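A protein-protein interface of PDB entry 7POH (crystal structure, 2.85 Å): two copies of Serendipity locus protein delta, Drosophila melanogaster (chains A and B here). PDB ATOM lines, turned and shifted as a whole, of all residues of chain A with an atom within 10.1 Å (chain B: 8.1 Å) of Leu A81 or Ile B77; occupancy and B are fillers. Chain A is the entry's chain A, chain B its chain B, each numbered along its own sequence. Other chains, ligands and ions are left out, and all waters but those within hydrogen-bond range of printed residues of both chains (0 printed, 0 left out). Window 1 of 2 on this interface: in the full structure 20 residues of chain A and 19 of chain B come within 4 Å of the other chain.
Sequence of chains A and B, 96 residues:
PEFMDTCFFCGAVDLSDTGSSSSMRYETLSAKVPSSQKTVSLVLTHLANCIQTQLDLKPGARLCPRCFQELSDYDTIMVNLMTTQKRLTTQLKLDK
The guanidinium group (NH1) of Arg A87 is in salt-bridge range of the side-chain carboxylate (OE2) of Glu B70 (2.6 Å). The side-chain amide nitrogen of Gln A85 sits at hydrogen-bond distance from the side-chain hydroxyl of Tyr B74, 2.9 Å away. The side-chain amide oxygen (OE1) of Gln A85 is in hydrogen-bond range of the side-chain sulfur (SG) of Cys B50 (3.5 Å).
The backbone carbonyl oxygen (O) of Thr A76 lies close to the side-chain amide oxygen (OD1) of Asn A80 (3.4 Å). The backbone carbonyl oxygen (O) of Lys A86 is in hydrogen-bond range of the side-chain hydroxyl (OG1) of Thr A89 (3.1 Å). The backbone carbonyl oxygen of His B46 sits close to the side-chain sulfur of Cys B50 (3.7 Å). The backbone carbonyl oxygen of Thr B76 sits close to the side-chain amide oxygen of Asn B80 (3.0 Å). The backbone carbonyl oxygen (O) of Asn B80 sits at hydrogen-bond distance from the side-chain hydroxyl (OG1) of Thr B84, at 2.5 Å. The backbone carbonyl oxygen (O) of Gln A85 sits close to the side-chain hydroxyl (OG1) of Thr A89.
Among the printed residues, merely in contact across the chains: Thr A84 with Tyr B74 (3.5 Å), Leu A81 with Tyr B74 (3.5 Å), Ile A77 with Thr B84 (3.5 Å), Leu A81 with Ile B77 (3.6 Å), Ile A77 with Leu B81 (3.6 Å), Thr A84 with Ile B77 (3.7 Å), Tyr A74 with Leu B81 (3.7 Å), Asn A80 with Ile B77 (3.7 Å), Leu A81 with Met B78 (3.7 Å), Thr A89 with Leu B47 (3.8 Å), Ile A77 with Ile B77 (3.8 Å), Leu A88 with Tyr B74 (3.8 Å), Ile A77 with Asn B80 (3.9 Å), Tyr A74 with Thr B84 (3.9 Å) and Leu A88 with Leu B47 (3.9 Å).
Printed residues of chain B within 4 Å of Ile A77: Ile B77, Asn B80, Leu B81 and Thr B84. Of the printed residues of chain B, Leu A81 touches Tyr B74 (3.5 Å), Ile B77 (3.6 Å) and Met B78 (3.7 Å). Printed residues of chain B within 4 Å of Thr A84: Tyr B74 and Ile B77. Of the printed residues of chain B, Gln A85 touches Cys B50 and Tyr B74. Of the printed residues of chain B, Thr A89 touches Leu B47 (3.8 Å). Ser B35 touches none of the printed residues of chain A. Of the printed residues of chain A, Cys B50 touches Gln A85. Asp B75 touches none of the printed residues of chain A. No residue of chain A comes within 4 Å of Thr B76. Ile B77 touches four residues of chain A. Of chain A, only Leu A81 comes within 4 Å of Met B78. Val B79 touches none of the printed residues of chain A. Of chain A, only Ile A77 comes within 4 Å of Asn B80. The nearest residue of chain B that does not touch Leu A81 is Leu B81 (5.0 Å). The nearest printed residue of chain A that does not touch Leu B47 is Gln A85 (4.1 Å).
Hydrophobic or aromatic side chains of chain A that line the printed part of chain B: Tyr A74, Ile A77, Leu A81 and Leu A88. Along chain A the printed residues that touch a printed residue of chain B span positions 74 to 89. Of the 19 printed residues of chain B, 9 touch a printed residue of chain A. Hydrophobic or aromatic side chains of chain B that line the printed part of chain A: Leu B47, Tyr B74, Ile B77 and Leu B81.
Tyr A74 touches Thr B84, and with the chains exchanged Thr A84 touches Tyr B74. Ile A77 touches Asn B80, and with the chains exchanged Asn A80 touches Ile B77. Ile A77 touches Leu B81, and with the chains exchanged Leu A81 touches Ile B77. Leu A81 touches Met B78, but with the chains exchanged Met A78 does not touch Leu B81 (4.1 Å). 13 positions are printed for both chains.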
ATOM      1  N   SER A  35      36.751 -15.950  21.128  1.00  0.00           N
ATOM      2  CA  SER A  35      35.452 -16.598  20.840  1.00  0.00           C
ATOM      3  C   SER A  35      35.199 -16.556  19.336  1.00  0.00           C
ATOM      4  O   SER A  35      35.034 -17.583  18.844  1.00  0.00           O
ATOM      5  CB  SER A  35      34.333 -16.005  21.643  1.00  0.00           C
ATOM      6  OG  SER A  35      34.654 -16.075  23.010  1.00  0.00           O
ATOM      7  N   ASP A  73      35.581  -9.958  26.038  1.00  0.00           N
ATOM      8  CA  ASP A  73      34.404 -10.431  26.814  1.00  0.00           C
ATOM      9  C   ASP A  73      33.112 -10.060  26.104  1.00  0.00           C
ATOM     10  O   ASP A  73      32.177 -10.897  26.114  1.00  0.00           O
ATOM     11  CB  ASP A  73      34.355  -9.854  28.220  1.00  0.00           C
ATOM     12  CG  ASP A  73      35.346 -10.500  29.147  1.00  0.00           C
ATOM     13  OD1 ASP A  73      35.917 -11.506  28.719  1.00  0.00           O
ATOM     14  OD2 ASP A  73      35.532  -9.985  30.285  1.00  0.00           O
ATOM     15  N   TYR A  74      33.062  -8.840  25.574  1.00  0.00           N
ATOM     16  CA  TYR A  74      31.958  -8.374  24.699  1.00  0.00           C
ATOM     17  C   TYR A  74      31.812  -9.342  23.526  1.00  0.00           C
ATOM     18  O   TYR A  74      30.711  -9.808  23.299  1.00  0.00           O
ATOM     19  CB  TYR A  74      32.222  -6.972  24.157  1.00  0.00           C
ATOM     20  CG  TYR A  74      31.146  -6.460  23.240  1.00  0.00           C
ATOM     21  CD1 TYR A  74      29.979  -5.944  23.745  1.00  0.00           C
ATOM     22  CD2 TYR A  74      31.302  -6.502  21.861  1.00  0.00           C
ATOM     23  CE1 TYR A  74      29.001  -5.451  22.890  1.00  0.00           C
ATOM     24  CE2 TYR A  74      30.333  -6.033  20.993  1.00  0.00           C
ATOM     25  CZ  TYR A  74      29.168  -5.493  21.508  1.00  0.00           C
ATOM     26  OH  TYR A  74      28.178  -5.023  20.680  1.00  0.00           O
ATOM     27  N   ASP A  75      32.889  -9.613  22.798  1.00  0.00           N
ATOM     28  CA  ASP A  75      32.800 -10.473  21.593  1.00  0.00           C
ATOM     29  C   ASP A  75      32.287 -11.847  22.047  1.00  0.00           C
ATOM     30  O   ASP A  75      31.445 -12.448  21.358  1.00  0.00           O
ATOM     31  CB  ASP A  75      34.131 -10.503  20.830  1.00  0.00           C
ATOM     32  CG  ASP A  75      34.336 -11.741  19.968  1.00  0.00           C
ATOM     33  OD1 ASP A  75      33.667 -11.796  18.917  1.00  0.00           O
ATOM     34  OD2 ASP A  75      35.162 -12.631  20.390  1.00  0.00           O
ATOM     35  N   THR A  76      32.756 -12.285  23.203  1.00  0.00           N
ATOM     36  CA  THR A  76      32.399 -13.585  23.802  1.00  0.00           C
ATOM     37  C   THR A  76      30.907 -13.551  24.108  1.00  0.00           C
ATOM     38  O   THR A  76      30.254 -14.426  23.614  1.00  0.00           O
ATOM     39  CB  THR A  76      33.342 -13.895  24.970  1.00  0.00           C
ATOM     40  OG1 THR A  76      34.655 -14.029  24.408  1.00  0.00           O
ATOM     41  CG2 THR A  76      32.934 -15.101  25.761  1.00  0.00           C
ATOM     42  N   ILE A  77      30.383 -12.538  24.804  1.00  0.00           N
ATOM     43  CA  ILE A  77      28.914 -12.402  25.085  1.00  0.00           C
ATOM     44  C   ILE A  77      28.153 -12.434  23.757  1.00  0.00           C
ATOM     45  O   ILE A  77      27.191 -13.156  23.669  1.00  0.00           O
ATOM     46  CB  ILE A  77      28.566 -11.111  25.858  1.00  0.00           C
ATOM     47  CG1 ILE A  77      29.169 -11.056  27.264  1.00  0.00           C
ATOM     48  CG2 ILE A  77      27.061 -10.921  25.956  1.00  0.00           C
ATOM     49  CD1 ILE A  77      29.457  -9.652  27.745  1.00  0.00           C
ATOM     50  N   MET A  78      28.576 -11.641  22.788  1.00  0.00           N
ATOM     51  CA  MET A  78      27.943 -11.498  21.457  1.00  0.00           C
ATOM     52  C   MET A  78      27.895 -12.876  20.778  1.00  0.00           C
ATOM     53  O   MET A  78      26.879 -13.196  20.171  1.00  0.00           O
ATOM     54  CB  MET A  78      28.723 -10.468  20.620  1.00  0.00           C
ATOM     55  CG  MET A  78      28.310 -10.314  19.178  1.00  0.00           C
ATOM     56  SD  MET A  78      26.615  -9.779  19.126  1.00  0.00           S
ATOM     57  CE  MET A  78      26.870  -8.021  19.378  1.00  0.00           C
ATOM     58  N   VAL A  79      28.937 -13.695  20.873  1.00  0.00           N
ATOM     59  CA  VAL A  79      28.935 -15.065  20.269  1.00  0.00           C
ATOM     60  C   VAL A  79      27.936 -15.939  21.026  1.00  0.00           C
ATOM     61  O   VAL A  79      27.185 -16.665  20.409  1.00  0.00           O
ATOM     62  CB  VAL A  79      30.310 -15.744  20.333  1.00  0.00           C
ATOM     63  CG1 VAL A  79      30.180 -17.211  20.016  1.00  0.00           C
ATOM     64  CG2 VAL A  79      31.379 -15.102  19.467  1.00  0.00           C
ATOM     65  N   ASN A  80      28.014 -15.991  22.346  1.00  0.00           N
ATOM     66  CA  ASN A  80      27.227 -17.001  23.085  1.00  0.00           C
ATOM     67  C   ASN A  80      25.773 -16.478  23.124  1.00  0.00           C
ATOM     68  O   ASN A  80      24.883 -17.304  23.184  1.00  0.00           O
ATOM     69  CB  ASN A  80      28.064 -17.571  24.248  1.00  0.00           C
ATOM     70  CG  ASN A  80      27.906 -16.836  25.544  1.00  0.00           C
ATOM     71  OD1 ASN A  80      28.876 -16.282  26.057  1.00  0.00           O
ATOM     72  ND2 ASN A  80      26.698 -16.857  26.083  1.00  0.00           N
ATOM     73  N   LEU A  81      25.503 -15.210  22.816  1.00  0.00           N
ATOM     74  CA  LEU A  81      24.106 -14.726  22.536  1.00  0.00           C
ATOM     75  C   LEU A  81      23.604 -15.281  21.198  1.00  0.00           C
ATOM     76  O   LEU A  81      22.488 -15.802  21.153  1.00  0.00           O
ATOM     77  CB  LEU A  81      24.073 -13.190  22.552  1.00  0.00           C
ATOM     78  CG  LEU A  81      22.727 -12.435  22.546  1.00  0.00           C
ATOM     79  CD1 LEU A  81      22.121 -12.378  21.186  1.00  0.00           C
ATOM     80  CD2 LEU A  81      21.699 -12.973  23.504  1.00  0.00           C
ATOM     81  N   MET A  82      24.381 -15.127  20.131  1.00  0.00           N
ATOM     82  CA  MET A  82      23.978 -15.560  18.766  1.00  0.00           C
ATOM     83  C   MET A  82      23.778 -17.084  18.761  1.00  0.00           C
ATOM     84  O   MET A  82      22.717 -17.523  18.258  1.00  0.00           O
ATOM     85  CB  MET A  82      24.986 -15.122  17.687  1.00  0.00           C
ATOM     86  CG  MET A  82      24.940 -13.658  17.330  1.00  0.00           C
ATOM     87  SD  MET A  82      23.222 -12.962  17.226  1.00  0.00           S
ATOM     88  CE  MET A  82      22.489 -14.050  16.000  1.00  0.00           C
ATOM     89  N   THR A  83      24.660 -17.860  19.394  1.00  0.00           N
ATOM     90  CA  THR A  83      24.522 -19.333  19.356  1.00  0.00           C
ATOM     91  C   THR A  83      23.303 -19.730  20.207  1.00  0.00           C
ATOM     92  O   THR A  83      22.418 -20.388  19.620  1.00  0.00           O
ATOM     93  CB  THR A  83      25.832 -20.095  19.579  1.00  0.00           C
ATOM     94  OG1 THR A  83      26.035 -20.229  20.967  1.00  0.00           O
ATOM     95  CG2 THR A  83      27.046 -19.473  18.922  1.00  0.00           C
ATOM     96  N   THR A  84      23.120 -19.252  21.450  1.00  0.00           N
ATOM     97  CA  THR A  84      21.923 -19.708  22.238  1.00  0.00           C
ATOM     98  C   THR A  84      20.638 -19.198  21.531  1.00  0.00           C
ATOM     99  O   THR A  84      19.582 -19.864  21.669  1.00  0.00           O
ATOM    100  CB  THR A  84      21.932 -19.561  23.783  1.00  0.00           C
ATOM    101  OG1 THR A  84      20.976 -18.586  24.178  1.00  0.00           O
ATOM    102  CG2 THR A  84      23.248 -19.342  24.502  1.00  0.00           C
ATOM    103  N   GLN A  85      20.714 -18.141  20.716  1.00  0.00           N
ATOM    104  CA  GLN A  85      19.525 -17.644  19.989  1.00  0.00           C
ATOM    105  C   GLN A  85      19.123 -18.672  18.932  1.00  0.00           C
ATOM    106  O   GLN A  85      17.921 -18.903  18.801  1.00  0.00           O
ATOM    107  CB  GLN A  85      19.766 -16.269  19.382  1.00  0.00           C
ATOM    108  CG  GLN A  85      18.462 -15.597  19.029  1.00  0.00           C
ATOM    109  CD  GLN A  85      18.671 -14.392  18.158  1.00  0.00           C
ATOM    110  OE1 GLN A  85      18.634 -14.480  16.937  1.00  0.00           O
ATOM    111  NE2 GLN A  85      18.836 -13.247  18.798  1.00  0.00           N
ATOM    112  N   LYS A  86      20.090 -19.266  18.228  1.00  0.00           N
ATOM    113  CA  LYS A  86      19.799 -20.274  17.176  1.00  0.00           C
ATOM    114  C   LYS A  86      19.281 -21.558  17.874  1.00  0.00           C
ATOM    115  O   LYS A  86      18.174 -22.086  17.468  1.00  0.00           O
ATOM    116  CB  LYS A  86      20.999 -20.465  16.233  1.00  0.00           C
ATOM    117  CG  LYS A  86      20.726 -21.486  15.127  1.00  0.00           C
ATOM    118  CD  LYS A  86      21.459 -21.369  13.786  1.00  0.00           C
ATOM    119  CE  LYS A  86      20.675 -20.693  12.662  1.00  0.00           C
ATOM    120  NZ  LYS A  86      19.458 -21.445  12.273  1.00  0.00           N
ATOM    121  N   ARG A  87      19.961 -22.028  18.932  1.00  0.00           N
ATOM    122  CA  ARG A  87      19.493 -23.218  19.678  1.00  0.00           C
ATOM    123  C   ARG A  87      17.997 -23.015  19.971  1.00  0.00           C
ATOM    124  O   ARG A  87      17.225 -23.928  19.663  1.00  0.00           O
ATOM    125  CB  ARG A  87      20.340 -23.513  20.915  1.00  0.00           C
ATOM    126  CG  ARG A  87      19.742 -24.626  21.766  1.00  0.00           C
ATOM    127  CD  ARG A  87      20.640 -25.420  22.706  1.00  0.00           C
ATOM    128  NE  ARG A  87      21.663 -24.578  23.287  1.00  0.00           N
ATOM    129  CZ  ARG A  87      21.491 -23.653  24.239  1.00  0.00           C
ATOM    130  NH1 ARG A  87      20.285 -23.426  24.747  1.00  0.00           N
ATOM    131  NH2 ARG A  87      22.540 -22.951  24.688  1.00  0.00           N
ATOM    132  N   LEU A  88      17.581 -21.838  20.443  1.00  0.00           N
ATOM    133  CA  LEU A  88      16.189 -21.622  20.923  1.00  0.00           C
ATOM    134  C   LEU A  88      15.216 -21.413  19.763  1.00  0.00           C
ATOM    135  O   LEU A  88      14.066 -21.885  19.866  1.00  0.00           O
ATOM    136  CB  LEU A  88      16.149 -20.441  21.894  1.00  0.00           C
ATOM    137  CG  LEU A  88      16.783 -20.699  23.261  1.00  0.00           C
ATOM    138  CD1 LEU A  88      16.554 -19.523  24.198  1.00  0.00           C
ATOM    139  CD2 LEU A  88      16.248 -21.968  23.888  1.00  0.00           C
ATOM    140  N   THR A  89      15.591 -20.677  18.725  1.00  0.00           N
ATOM    141  CA  THR A  89      14.668 -20.459  17.586  1.00  0.00           C
ATOM    142  C   THR A  89      14.476 -21.802  16.890  1.00  0.00           C
ATOM    143  O   THR A  89      13.329 -22.087  16.620  1.00  0.00           O
ATOM    144  CB  THR A  89      15.147 -19.428  16.569  1.00  0.00           C
ATOM    145  OG1 THR A  89      16.365 -19.975  16.075  1.00  0.00           O
ATOM    146  CG2 THR A  89      15.331 -18.046  17.151  1.00  0.00           C
ATOM    147  N   SER B  35      16.757 -11.741  35.533  1.00  0.00           N
ATOM    148  CA  SER B  35      17.823 -10.729  35.434  1.00  0.00           C
ATOM    149  C   SER B  35      17.364  -9.664  34.429  1.00  0.00           C
ATOM    150  O   SER B  35      18.161  -9.313  33.579  1.00  0.00           O
ATOM    151  CB  SER B  35      19.166 -11.430  35.095  1.00  0.00           C
ATOM    152  OG  SER B  35      19.064 -12.181  33.903  1.00  0.00           O
ATOM    153  N   HIS B  46       9.776 -12.332  21.372  1.00  0.00           N
ATOM    154  CA  HIS B  46      11.104 -11.948  20.827  1.00  0.00           C
ATOM    155  C   HIS B  46      11.660 -13.060  19.921  1.00  0.00           C
ATOM    156  O   HIS B  46      12.014 -12.770  18.747  1.00  0.00           O
ATOM    157  CB  HIS B  46      12.063 -11.500  21.938  1.00  0.00           C
ATOM    158  CG  HIS B  46      13.480 -11.407  21.480  1.00  0.00           C
ATOM    159  ND1 HIS B  46      13.833 -10.942  20.223  1.00  0.00           N
ATOM    160  CD2 HIS B  46      14.628 -11.739  22.089  1.00  0.00           C
ATOM    161  CE1 HIS B  46      15.133 -11.005  20.082  1.00  0.00           C
ATOM    162  NE2 HIS B  46      15.639 -11.499  21.204  1.00  0.00           N
ATOM    163  N   LEU B  47      11.719 -14.296  20.407  1.00  0.00           N
ATOM    164  CA  LEU B  47      12.327 -15.409  19.623  1.00  0.00           C
ATOM    165  C   LEU B  47      11.514 -15.679  18.350  1.00  0.00           C
ATOM    166  O   LEU B  47      12.131 -16.041  17.325  1.00  0.00           O
ATOM    167  CB  LEU B  47      12.460 -16.661  20.495  1.00  0.00           C
ATOM    168  CG  LEU B  47      13.548 -16.583  21.567  1.00  0.00           C
ATOM    169  CD1 LEU B  47      13.403 -17.712  22.580  1.00  0.00           C
ATOM    170  CD2 LEU B  47      14.936 -16.594  20.935  1.00  0.00           C
ATOM    171  N   CYS B  50      12.590 -13.240  15.677  1.00  0.00           N
ATOM    172  CA  CYS B  50      13.902 -13.580  15.079  1.00  0.00           C
ATOM    173  C   CYS B  50      13.741 -14.474  13.835  1.00  0.00           C
ATOM    174  O   CYS B  50      14.568 -14.317  12.940  1.00  0.00           O
ATOM    175  CB  CYS B  50      14.859 -14.185  16.096  1.00  0.00           C
ATOM    176  SG  CYS B  50      15.443 -12.987  17.317  1.00  0.00           S
ATOM    177  N   GLU B  70      16.218 -22.104  30.482  1.00  0.00           N
ATOM    178  CA  GLU B  70      16.978 -21.853  29.227  1.00  0.00           C
ATOM    179  C   GLU B  70      16.601 -20.452  28.694  1.00  0.00           C
ATOM    180  O   GLU B  70      17.490 -19.654  28.409  1.00  0.00           O
ATOM    181  CB  GLU B  70      16.801 -23.028  28.238  1.00  0.00           C
ATOM    182  CG  GLU B  70      18.040 -23.318  27.370  1.00  0.00           C
ATOM    183  CD  GLU B  70      18.575 -24.741  27.379  1.00  0.00           C
ATOM    184  OE1 GLU B  70      18.269 -25.531  28.311  1.00  0.00           O
ATOM    185  OE2 GLU B  70      19.338 -25.076  26.456  1.00  0.00           O
ATOM    186  N   LEU B  71      15.329 -20.101  28.696  1.00  0.00           N
ATOM    187  CA  LEU B  71      14.863 -18.730  28.346  1.00  0.00           C
ATOM    188  C   LEU B  71      15.380 -17.701  29.368  1.00  0.00           C
ATOM    189  O   LEU B  71      15.771 -16.609  28.917  1.00  0.00           O
ATOM    190  CB  LEU B  71      13.335 -18.737  28.304  1.00  0.00           C
ATOM    191  CG  LEU B  71      12.721 -19.703  27.293  1.00  0.00           C
ATOM    192  CD1 LEU B  71      11.315 -20.083  27.714  1.00  0.00           C
ATOM    193  CD2 LEU B  71      12.734 -19.123  25.886  1.00  0.00           C
ATOM    194  N   SER B  72      15.366 -18.028  30.671  1.00  0.00           N
ATOM    195  CA  SER B  72      15.928 -17.189  31.752  1.00  0.00           C
ATOM    196  C   SER B  72      17.374 -16.807  31.396  1.00  0.00           C
ATOM    197  O   SER B  72      17.717 -15.597  31.421  1.00  0.00           O
ATOM    198  CB  SER B  72      15.823 -17.840  33.132  1.00  0.00           C
ATOM    199  OG  SER B  72      14.503 -17.756  33.684  1.00  0.00           O
ATOM    200  N   ASP B  73      18.180 -17.775  30.992  1.00  0.00           N
ATOM    201  CA  ASP B  73      19.622 -17.562  30.690  1.00  0.00           C
ATOM    202  C   ASP B  73      19.843 -16.784  29.400  1.00  0.00           C
ATOM    203  O   ASP B  73      20.850 -16.099  29.311  1.00  0.00           O
ATOM    204  CB  ASP B  73      20.405 -18.854  30.475  1.00  0.00           C
ATOM    205  CG  ASP B  73      20.388 -19.761  31.674  1.00  0.00           C
ATOM    206  OD1 ASP B  73      20.157 -19.235  32.783  1.00  0.00           O
ATOM    207  OD2 ASP B  73      20.511 -20.974  31.463  1.00  0.00           O
ATOM    208  N   TYR B  74      19.045 -16.994  28.377  1.00  0.00           N
ATOM    209  CA  TYR B  74      19.156 -16.173  27.150  1.00  0.00           C
ATOM    210  C   TYR B  74      18.963 -14.725  27.589  1.00  0.00           C
ATOM    211  O   TYR B  74      19.771 -13.838  27.252  1.00  0.00           O
ATOM    212  CB  TYR B  74      18.124 -16.620  26.133  1.00  0.00           C
ATOM    213  CG  TYR B  74      18.023 -15.743  24.923  1.00  0.00           C
ATOM    214  CD1 TYR B  74      19.023 -15.715  23.966  1.00  0.00           C
ATOM    215  CD2 TYR B  74      16.886 -14.988  24.690  1.00  0.00           C
ATOM    216  CE1 TYR B  74      18.896 -14.941  22.814  1.00  0.00           C
ATOM    217  CE2 TYR B  74      16.749 -14.211  23.546  1.00  0.00           C
ATOM    218  CZ  TYR B  74      17.758 -14.177  22.601  1.00  0.00           C
ATOM    219  OH  TYR B  74      17.615 -13.413  21.474  1.00  0.00           O
ATOM    220  N   ASP B  75      17.946 -14.515  28.418  1.00  0.00           N
ATOM    221  CA  ASP B  75      17.581 -13.164  28.909  1.00  0.00           C
ATOM    222  C   ASP B  75      18.784 -12.605  29.671  1.00  0.00           C
ATOM    223  O   ASP B  75      19.200 -11.452  29.370  1.00  0.00           O
ATOM    224  CB  ASP B  75      16.281 -13.208  29.704  1.00  0.00           C
ATOM    225  CG  ASP B  75      16.074 -11.950  30.486  1.00  0.00           C
ATOM    226  OD1 ASP B  75      15.628 -10.965  29.823  1.00  0.00           O
ATOM    227  OD2 ASP B  75      16.380 -12.003  31.737  1.00  0.00           O
ATOM    228  N   THR B  76      19.367 -13.423  30.541  1.00  0.00           N
ATOM    229  CA  THR B  76      20.590 -13.050  31.290  1.00  0.00           C
ATOM    230  C   THR B  76      21.728 -12.652  30.342  1.00  0.00           C
ATOM    231  O   THR B  76      22.295 -11.607  30.601  1.00  0.00           O
ATOM    232  CB  THR B  76      21.035 -14.166  32.229  1.00  0.00           C
ATOM    233  OG1 THR B  76      19.861 -14.702  32.848  1.00  0.00           O
ATOM    234  CG2 THR B  76      22.038 -13.680  33.249  1.00  0.00           C
ATOM    235  N   ILE B  77      21.961 -13.364  29.231  1.00  0.00           N
ATOM    236  CA  ILE B  77      23.034 -13.039  28.237  1.00  0.00           C
ATOM    237  C   ILE B  77      22.740 -11.696  27.568  1.00  0.00           C
ATOM    238  O   ILE B  77      23.617 -10.790  27.599  1.00  0.00           O
ATOM    239  CB  ILE B  77      23.180 -14.129  27.173  1.00  0.00           C
ATOM    240  CG1 ILE B  77      23.557 -15.478  27.791  1.00  0.00           C
ATOM    241  CG2 ILE B  77      24.203 -13.719  26.121  1.00  0.00           C
ATOM    242  CD1 ILE B  77      23.092 -16.640  26.983  1.00  0.00           C
ATOM    243  N   MET B  78      21.559 -11.576  26.972  1.00  0.00           N
ATOM    244  CA  MET B  78      21.083 -10.306  26.368  1.00  0.00           C
ATOM    245  C   MET B  78      21.340  -9.127  27.328  1.00  0.00           C
ATOM    246  O   MET B  78      21.775  -8.070  26.824  1.00  0.00           O
ATOM    247  CB  MET B  78      19.601 -10.430  26.064  1.00  0.00           C
ATOM    248  CG  MET B  78      18.951  -9.180  25.543  1.00  0.00           C
ATOM    249  SD  MET B  78      19.163  -9.058  23.815  1.00  0.00           S
ATOM    250  CE  MET B  78      18.103 -10.395  23.257  1.00  0.00           C
ATOM    251  N   VAL B  79      21.118  -9.280  28.641  1.00  0.00           N
ATOM    252  CA  VAL B  79      21.326  -8.169  29.628  1.00  0.00           C
ATOM    253  C   VAL B  79      22.823  -7.840  29.767  1.00  0.00           C
ATOM    254  O   VAL B  79      23.198  -6.642  29.882  1.00  0.00           O
ATOM    255  CB  VAL B  79      20.675  -8.502  30.985  1.00  0.00           C
ATOM    256  CG1 VAL B  79      21.172  -7.618  32.115  1.00  0.00           C
ATOM    257  CG2 VAL B  79      19.158  -8.451  30.864  1.00  0.00           C
ATOM    258  N   ASN B  80      23.662  -8.862  29.794  1.00  0.00           N
ATOM    259  CA  ASN B  80      25.121  -8.660  29.819  1.00  0.00           C
ATOM    260  C   ASN B  80      25.558  -8.029  28.499  1.00  0.00           C
ATOM    261  O   ASN B  80      26.489  -7.237  28.551  1.00  0.00           O
ATOM    262  CB  ASN B  80      25.837  -9.955  30.139  1.00  0.00           C
ATOM    263  CG  ASN B  80      25.738 -10.255  31.609  1.00  0.00           C
ATOM    264  OD1 ASN B  80      24.716 -10.702  32.066  1.00  0.00           O
ATOM    265  ND2 ASN B  80      26.796  -9.993  32.352  1.00  0.00           N
ATOM    266  N   LEU B  81      24.873  -8.285  27.387  1.00  0.00           N
ATOM    267  CA  LEU B  81      25.113  -7.503  26.148  1.00  0.00           C
ATOM    268  C   LEU B  81      24.661  -6.050  26.372  1.00  0.00           C
ATOM    269  O   LEU B  81      25.536  -5.185  26.194  1.00  0.00           O
ATOM    270  CB  LEU B  81      24.412  -8.181  24.972  1.00  0.00           C
ATOM    271  CG  LEU B  81      25.078  -8.100  23.604  1.00  0.00           C
ATOM    272  CD1 LEU B  81      24.678  -6.851  22.882  1.00  0.00           C
ATOM    273  CD2 LEU B  81      26.583  -8.172  23.664  1.00  0.00           C
ATOM    274  N   MET B  82      23.412  -5.788  26.821  1.00  0.00           N
ATOM    275  CA  MET B  82      22.851  -4.410  26.979  1.00  0.00           C
ATOM    276  C   MET B  82      23.925  -3.591  27.699  1.00  0.00           C
ATOM    277  O   MET B  82      24.357  -2.522  27.158  1.00  0.00           O
ATOM    278  CB  MET B  82      21.534  -4.336  27.788  1.00  0.00           C
ATOM    279  CG  MET B  82      20.173  -4.268  26.990  1.00  0.00           C
ATOM    280  SD  MET B  82      18.866  -5.584  27.427  1.00  0.00           S
ATOM    281  CE  MET B  82      17.471  -5.268  26.331  1.00  0.00           C
ATOM    282  N   THR B  83      24.395  -4.089  28.852  1.00  0.00           N
ATOM    283  CA  THR B  83      25.133  -3.252  29.838  1.00  0.00           C
ATOM    284  C   THR B  83      26.584  -3.103  29.385  1.00  0.00           C
ATOM    285  O   THR B  83      27.131  -1.948  29.488  1.00  0.00           O
ATOM    286  CB  THR B  83      25.083  -3.809  31.259  1.00  0.00           C
ATOM    287  OG1 THR B  83      25.874  -4.990  31.279  1.00  0.00           O
ATOM    288  CG2 THR B  83      23.689  -4.099  31.757  1.00  0.00           C
ATOM    289  N   THR B  84      27.182  -4.208  28.906  1.00  0.00           N
ATOM    290  CA  THR B  84      28.571  -4.202  28.392  1.00  0.00           C
ATOM    291  C   THR B  84      28.659  -3.202  27.250  1.00  0.00           C
ATOM    292  O   THR B  84      29.572  -2.331  27.292  1.00  0.00           O
ATOM    293  CB  THR B  84      29.036  -5.567  27.923  1.00  0.00           C
ATOM    294  OG1 THR B  84      28.769  -6.458  29.003  1.00  0.00           O
ATOM    295  CG2 THR B  84      30.513  -5.599  27.606  1.00  0.00           C
